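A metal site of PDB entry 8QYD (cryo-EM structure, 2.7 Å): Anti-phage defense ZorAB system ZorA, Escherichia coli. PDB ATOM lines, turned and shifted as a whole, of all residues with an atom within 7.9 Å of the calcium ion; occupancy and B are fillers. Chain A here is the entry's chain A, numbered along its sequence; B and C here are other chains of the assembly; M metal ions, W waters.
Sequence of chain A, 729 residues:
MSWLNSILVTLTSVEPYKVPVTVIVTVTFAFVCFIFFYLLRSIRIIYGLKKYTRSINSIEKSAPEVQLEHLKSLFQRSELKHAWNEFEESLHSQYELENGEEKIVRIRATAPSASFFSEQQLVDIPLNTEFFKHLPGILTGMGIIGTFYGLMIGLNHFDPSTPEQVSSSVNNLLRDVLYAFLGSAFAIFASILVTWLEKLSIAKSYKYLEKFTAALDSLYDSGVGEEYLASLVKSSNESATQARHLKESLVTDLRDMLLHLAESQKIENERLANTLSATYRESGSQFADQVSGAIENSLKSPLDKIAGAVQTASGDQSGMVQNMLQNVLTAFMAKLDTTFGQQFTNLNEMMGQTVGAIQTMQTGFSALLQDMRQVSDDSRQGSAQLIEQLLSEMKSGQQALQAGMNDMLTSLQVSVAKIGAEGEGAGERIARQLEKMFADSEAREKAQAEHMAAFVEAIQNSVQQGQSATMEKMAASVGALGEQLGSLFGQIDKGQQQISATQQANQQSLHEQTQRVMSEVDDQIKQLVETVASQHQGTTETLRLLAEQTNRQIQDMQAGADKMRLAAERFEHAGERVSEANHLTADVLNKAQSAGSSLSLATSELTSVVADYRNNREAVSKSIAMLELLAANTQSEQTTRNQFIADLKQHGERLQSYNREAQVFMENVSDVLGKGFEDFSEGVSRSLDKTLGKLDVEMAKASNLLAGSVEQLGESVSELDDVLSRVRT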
ATOM      1  N   HIS A  82      26.339  36.122 -23.557  1.00  0.00           N
ATOM      2  CA  HIS A  82      26.228  34.864 -22.832  1.00  0.00           C
ATOM      3  C   HIS A  82      25.334  33.876 -23.569  1.00  0.00           C
ATOM      4  O   HIS A  82      25.652  32.676 -23.641  1.00  0.00           O
ATOM      5  CB  HIS A  82      25.686  35.122 -21.425  1.00  0.00           C
ATOM      6  CG  HIS A  82      25.327  33.880 -20.682  1.00  0.00           C
ATOM      7  ND1 HIS A  82      26.267  33.018 -20.171  1.00  0.00           N
ATOM      8  CD2 HIS A  82      24.114  33.355 -20.367  1.00  0.00           C
ATOM      9  CE1 HIS A  82      25.653  32.008 -19.562  1.00  0.00           C
ATOM     10  NE2 HIS A  82      24.355  32.191 -19.681  1.00  0.00           N
ATOM     11  N   ASN A  85      27.307  32.426 -26.413  1.00  0.00           N
ATOM     12  CA  ASN A  85      28.312  31.472 -25.951  1.00  0.00           C
ATOM     13  C   ASN A  85      27.676  30.135 -25.634  1.00  0.00           C
ATOM     14  O   ASN A  85      28.175  29.073 -26.053  1.00  0.00           O
ATOM     15  CB  ASN A  85      29.054  32.030 -24.736  1.00  0.00           C
ATOM     16  CG  ASN A  85      30.001  33.153 -25.094  1.00  0.00           C
ATOM     17  OD1 ASN A  85      30.463  33.243 -26.231  1.00  0.00           O
ATOM     18  ND2 ASN A  85      30.308  33.994 -24.122  1.00  0.00           N
ATOM     19  N   GLU A  86      26.549  30.145 -24.924  1.00  0.00           N
ATOM     20  CA  GLU A  86      25.862  28.902 -24.597  1.00  0.00           C
ATOM     21  C   GLU A  86      25.343  28.208 -25.861  1.00  0.00           C
ATOM     22  O   GLU A  86      25.446  26.985 -25.995  1.00  0.00           O
ATOM     23  CB  GLU A  86      24.732  29.174 -23.616  1.00  0.00           C
ATOM     24  CG  GLU A  86      25.197  29.778 -22.318  1.00  0.00           C
ATOM     25  CD  GLU A  86      26.277  28.952 -21.649  1.00  0.00           C
ATOM     26  OE1 GLU A  86      26.084  27.719 -21.518  1.00  0.00           O
ATOM     27  OE2 GLU A  86      27.317  29.514 -21.263  1.00  0.00           O
ATOM     28  N   PHE A  87      24.775  28.983 -26.788  1.00  0.00           N
ATOM     29  CA  PHE A  87      24.266  28.395 -28.024  1.00  0.00           C
ATOM     30  C   PHE A  87      25.380  27.769 -28.844  1.00  0.00           C
ATOM     31  O   PHE A  87      25.222  26.679 -29.390  1.00  0.00           O
ATOM     32  CB  PHE A  87      23.531  29.458 -28.828  1.00  0.00           C
ATOM     33  CG  PHE A  87      22.973  28.967 -30.120  1.00  0.00           C
ATOM     34  CD1 PHE A  87      22.066  27.923 -30.147  1.00  0.00           C
ATOM     35  CD2 PHE A  87      23.317  29.561 -31.319  1.00  0.00           C
ATOM     36  CE1 PHE A  87      21.534  27.473 -31.331  1.00  0.00           C
ATOM     37  CE2 PHE A  87      22.798  29.113 -32.508  1.00  0.00           C
ATOM     38  CZ  PHE A  87      21.908  28.076 -32.510  1.00  0.00           C
ATOM     39  N   GLU A  89      28.076  26.568 -27.613  1.00  0.00           N
ATOM     40  CA  GLU A  89      28.355  25.308 -26.932  1.00  0.00           C
ATOM     41  C   GLU A  89      27.374  24.220 -27.383  1.00  0.00           C
ATOM     42  O   GLU A  89      27.764  23.049 -27.518  1.00  0.00           O
ATOM     43  CB  GLU A  89      28.288  25.480 -25.419  1.00  0.00           C
ATOM     44  CG  GLU A  89      29.368  26.352 -24.835  1.00  0.00           C
ATOM     45  CD  GLU A  89      29.235  26.491 -23.339  1.00  0.00           C
ATOM     46  OE1 GLU A  89      28.223  26.018 -22.793  1.00  0.00           O
ATOM     47  OE2 GLU A  89      30.131  27.099 -22.720  1.00  0.00           O
ATOM     48  N   SER A  90      26.116  24.586 -27.606  1.00  0.00           N
ATOM     49  CA  SER A  90      25.145  23.584 -28.051  1.00  0.00           C
ATOM     50  C   SER A  90      25.444  23.072 -29.452  1.00  0.00           C
ATOM     51  O   SER A  90      25.142  21.921 -29.764  1.00  0.00           O
ATOM     52  CB  SER A  90      23.738  24.157 -27.996  1.00  0.00           C
ATOM     53  OG  SER A  90      23.532  25.100 -29.032  1.00  0.00           O
ATOM     54  N   PHE A 116      18.436  29.266 -25.492  1.00  0.00           N
ATOM     55  CA  PHE A 116      19.435  30.162 -24.950  1.00  0.00           C
ATOM     56  C   PHE A 116      19.094  31.631 -25.184  1.00  0.00           C
ATOM     57  O   PHE A 116      19.359  32.458 -24.313  1.00  0.00           O
ATOM     58  CB  PHE A 116      20.799  29.856 -25.563  1.00  0.00           C
ATOM     59  CG  PHE A 116      21.116  28.385 -25.590  1.00  0.00           C
ATOM     60  CD1 PHE A 116      21.635  27.763 -24.470  1.00  0.00           C
ATOM     61  CD2 PHE A 116      20.860  27.637 -26.714  1.00  0.00           C
ATOM     62  CE1 PHE A 116      21.912  26.417 -24.491  1.00  0.00           C
ATOM     63  CE2 PHE A 116      21.137  26.290 -26.736  1.00  0.00           C
ATOM     64  CZ  PHE A 116      21.662  25.676 -25.619  1.00  0.00           C
ATOM     65  N   ARG B 108      32.524  19.051 -18.137  1.00  0.00           N
ATOM     66  CA  ARG B 108      31.495  19.386 -19.107  1.00  0.00           C
ATOM     67  C   ARG B 108      30.141  19.485 -18.422  1.00  0.00           C
ATOM     68  O   ARG B 108      29.857  18.733 -17.486  1.00  0.00           O
ATOM     69  CB  ARG B 108      31.442  18.342 -20.217  1.00  0.00           C
ATOM     70  CG  ARG B 108      32.784  18.013 -20.831  1.00  0.00           C
ATOM     71  CD  ARG B 108      33.321  19.178 -21.626  1.00  0.00           C
ATOM     72  NE  ARG B 108      32.470  19.518 -22.757  1.00  0.00           N
ATOM     73  CZ  ARG B 108      32.603  19.024 -23.980  1.00  0.00           C
ATOM     74  NH1 ARG B 108      33.552  18.150 -24.275  1.00  0.00           N
ATOM     75  NH2 ARG B 108      31.774  19.417 -24.937  1.00  0.00           N
ATOM     76  N   ALA B 109      29.319  20.411 -18.896  1.00  0.00           N
ATOM     77  CA  ALA B 109      27.976  20.594 -18.368  1.00  0.00           C
ATOM     78  C   ALA B 109      26.995  19.786 -19.199  1.00  0.00           C
ATOM     79  O   ALA B 109      26.979  19.876 -20.429  1.00  0.00           O
ATOM     80  CB  ALA B 109      27.583  22.074 -18.374  1.00  0.00           C
ATOM     81  N   ALA B 111      23.546  19.682 -18.070  1.00  0.00           N
ATOM     82  CA  ALA B 111      22.285  20.377 -17.861  1.00  0.00           C
ATOM     83  C   ALA B 111      22.575  21.816 -17.492  1.00  0.00           C
ATOM     84  O   ALA B 111      23.635  22.112 -16.918  1.00  0.00           O
ATOM     85  CB  ALA B 111      21.449  19.717 -16.749  1.00  0.00           C
ATOM     86  N   PRO B 112      21.671  22.739 -17.812  1.00  0.00           N
ATOM     87  CA  PRO B 112      21.881  24.135 -17.409  1.00  0.00           C
ATOM     88  C   PRO B 112      21.832  24.280 -15.894  1.00  0.00           C
ATOM     89  O   PRO B 112      21.138  23.545 -15.198  1.00  0.00           O
ATOM     90  CB  PRO B 112      20.711  24.876 -18.073  1.00  0.00           C
ATOM     91  CG  PRO B 112      19.680  23.827 -18.286  1.00  0.00           C
ATOM     92  CD  PRO B 112      20.424  22.567 -18.569  1.00  0.00           C
ATOM     93  N   THR B 213      23.196  32.230 -12.302  1.00  0.00           N
ATOM     94  CA  THR B 213      23.212  31.004 -13.083  1.00  0.00           C
ATOM     95  C   THR B 213      23.956  31.172 -14.392  1.00  0.00           C
ATOM     96  O   THR B 213      24.570  30.221 -14.882  1.00  0.00           O
ATOM     97  CB  THR B 213      21.792  30.500 -13.353  1.00  0.00           C
ATOM     98  OG1 THR B 213      21.034  31.522 -14.017  1.00  0.00           O
ATOM     99  CG2 THR B 213      21.104  30.131 -12.044  1.00  0.00           C
ATOM    100  N   ALA B 214      23.912  32.371 -14.987  1.00  0.00           N
ATOM    101  CA  ALA B 214      24.715  32.639 -16.170  1.00  0.00           C
ATOM    102  C   ALA B 214      26.200  32.565 -15.837  1.00  0.00           C
ATOM    103  O   ALA B 214      26.993  32.040 -16.632  1.00  0.00           O
ATOM    104  CB  ALA B 214      24.377  34.011 -16.730  1.00  0.00           C
ATOM    105  N   ALA B 215      26.595  33.074 -14.672  1.00  0.00           N
ATOM    106  CA  ALA B 215      27.981  32.926 -14.243  1.00  0.00           C
ATOM    107  C   ALA B 215      28.355  31.461 -14.077  1.00  0.00           C
ATOM    108  O   ALA B 215      29.441  31.042 -14.497  1.00  0.00           O
ATOM    109  CB  ALA B 215      28.209  33.688 -12.944  1.00  0.00           C
ATOM    110  N   LEU B 216      27.472  30.670 -13.475  1.00  0.00           N
ATOM    111  CA  LEU B 216      27.742  29.240 -13.331  1.00  0.00           C
ATOM    112  C   LEU B 216      27.762  28.534 -14.669  1.00  0.00           C
ATOM    113  O   LEU B 216      28.587  27.635 -14.901  1.00  0.00           O
ATOM    114  CB  LEU B 216      26.720  28.599 -12.402  1.00  0.00           C
ATOM    115  CG  LEU B 216      27.182  28.362 -10.967  1.00  0.00           C
ATOM    116  CD1 LEU B 216      26.130  27.610 -10.209  1.00  0.00           C
ATOM    117  CD2 LEU B 216      28.494  27.615 -10.938  1.00  0.00           C
ATOM    118  N   ASP B 217      26.848  28.891 -15.578  1.00  0.00           N
ATOM    119  CA  ASP B 217      26.784  28.248 -16.882  1.00  0.00           C
ATOM    120  C   ASP B 217      28.037  28.507 -17.711  1.00  0.00           C
ATOM    121  O   ASP B 217      28.412  27.688 -18.557  1.00  0.00           O
ATOM    122  CB  ASP B 217      25.551  28.717 -17.647  1.00  0.00           C
ATOM    123  CG  ASP B 217      24.330  27.900 -17.327  1.00  0.00           C
ATOM    124  OD1 ASP B 217      24.479  26.756 -16.874  1.00  0.00           O
ATOM    125  OD2 ASP B 217      23.207  28.412 -17.543  1.00  0.00           O
ATOM    126  N   SER B 218      28.703  29.647 -17.486  1.00  0.00           N
ATOM    127  CA  SER B 218      29.847  30.011 -18.292  1.00  0.00           C
ATOM    128  C   SER B 218      31.095  29.214 -17.932  1.00  0.00           C
ATOM    129  O   SER B 218      32.045  29.185 -18.719  1.00  0.00           O
ATOM    130  CB  SER B 218      30.145  31.500 -18.154  1.00  0.00           C
ATOM    131  OG  SER B 218      30.818  31.761 -16.930  1.00  0.00           O
ATOM    132  N   LEU B 219      31.109  28.565 -16.774  1.00  0.00           N
ATOM    133  CA  LEU B 219      32.313  27.848 -16.353  1.00  0.00           C
ATOM    134  C   LEU B 219      32.519  26.567 -17.136  1.00  0.00           C
ATOM    135  O   LEU B 219      33.664  26.131 -17.309  1.00  0.00           O
ATOM    136  CB  LEU B 219      32.232  27.530 -14.853  1.00  0.00           C
ATOM    137  CG  LEU B 219      32.441  28.675 -13.863  1.00  0.00           C
ATOM    138  CD1 LEU B 219      32.365  28.154 -12.452  1.00  0.00           C
ATOM    139  CD2 LEU B 219      33.773  29.343 -14.099  1.00  0.00           C
ATOM    140  N   TYR B 220      31.452  25.941 -17.618  1.00  0.00           N
ATOM    141  CA  TYR B 220      31.518  24.614 -18.192  1.00  0.00           C
ATOM    142  C   TYR B 220      30.855  24.585 -19.562  1.00  0.00           C
ATOM    143  O   TYR B 220      29.947  25.379 -19.847  1.00  0.00           O
ATOM    144  CB  TYR B 220      30.870  23.592 -17.265  1.00  0.00           C
ATOM    145  CG  TYR B 220      31.450  23.642 -15.870  1.00  0.00           C
ATOM    146  CD1 TYR B 220      32.721  23.148 -15.608  1.00  0.00           C
ATOM    147  CD2 TYR B 220      30.733  24.193 -14.815  1.00  0.00           C
ATOM    148  CE1 TYR B 220      33.259  23.198 -14.349  1.00  0.00           C
ATOM    149  CE2 TYR B 220      31.265  24.236 -13.553  1.00  0.00           C
ATOM    150  CZ  TYR B 220      32.531  23.749 -13.321  1.00  0.00           C
ATOM    151  OH  TYR B 220      33.063  23.792 -12.059  1.00  0.00           O
ATOM    152  N   ASP B 221      31.307  23.658 -20.396  1.00  0.00           N
ATOM    153  CA  ASP B 221      30.860  23.548 -21.780  1.00  0.00           C
ATOM    154  C   ASP B 221      29.987  22.311 -21.950  1.00  0.00           C
ATOM    155  O   ASP B 221      30.195  21.301 -21.273  1.00  0.00           O
ATOM    156  CB  ASP B 221      32.048  23.486 -22.743  1.00  0.00           C
ATOM    157  CG  ASP B 221      32.729  24.823 -22.916  1.00  0.00           C
ATOM    158  OD1 ASP B 221      32.773  25.594 -21.942  1.00  0.00           O
ATOM    159  OD2 ASP B 221      33.224  25.093 -24.025  1.00  0.00           O
ATOM    160  N   SER B 222      29.029  22.388 -22.862  1.00  0.00           N
ATOM    161  CA  SER B 222      28.102  21.306 -23.129  1.00  0.00           C
ATOM    162  C   SER B 222      28.492  20.578 -24.415  1.00  0.00           C
ATOM    163  O   SER B 222      29.539  20.836 -25.018  1.00  0.00           O
ATOM    164  CB  SER B 222      26.682  21.860 -23.199  1.00  0.00           C
ATOM    165  OG  SER B 222      26.386  22.613 -22.050  1.00  0.00           O
ATOM    166  N   PHE C   6      18.813  21.017 -22.536  1.00  0.00           N
ATOM    167  CA  PHE C   6      18.789  22.436 -22.849  1.00  0.00           C
ATOM    168  C   PHE C   6      17.595  22.734 -23.760  1.00  0.00           C
ATOM    169  O   PHE C   6      17.725  22.998 -24.954  1.00  0.00           O
ATOM    170  CB  PHE C   6      20.108  22.879 -23.479  1.00  0.00           C
ATOM    171  CG  PHE C   6      21.306  22.631 -22.602  1.00  0.00           C
ATOM    172  CD1 PHE C   6      21.892  21.378 -22.526  1.00  0.00           C
ATOM    173  CD2 PHE C   6      21.857  23.655 -21.852  1.00  0.00           C
ATOM    174  CE1 PHE C   6      22.980  21.152 -21.723  1.00  0.00           C
ATOM    175  CE2 PHE C   6      22.951  23.437 -21.051  1.00  0.00           C
ATOM    176  CZ  PHE C   6      23.516  22.182 -20.988  1.00  0.00           C
HETATM  177 CA    CA M   1      28.387  26.724 -20.666  1.00  0.00          CA
HETATM  178  O   HOH W   1      27.000  25.491 -19.417  1.00  0.00           O
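The calcium ion is bound by the backbone carbonyl oxygen (O) of Tyr 220 of chain B (2.2 Å), water W1 (2.2 Å), the side-chain carboxylate (OE1) of Glu 89 (2.2 Å), the backbone carbonyl oxygen (O) of Asp 217 of chain B (2.3 Å), the side-chain carboxylate (OE1) of Glu 86 (2.6 Å) and the side-chain carboxylate (OE2) of Glu 89 (2.7 Å).
Slightly farther from the calcium ion lies OE2 of Glu 86 (3.0 Å).
Along chain A the residues within 4 Å of the calcium ion span positions 86 to 89.
The nearest printed residue that does not touch the calcium ion is Asp 221 of chain B (4.2 Å).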
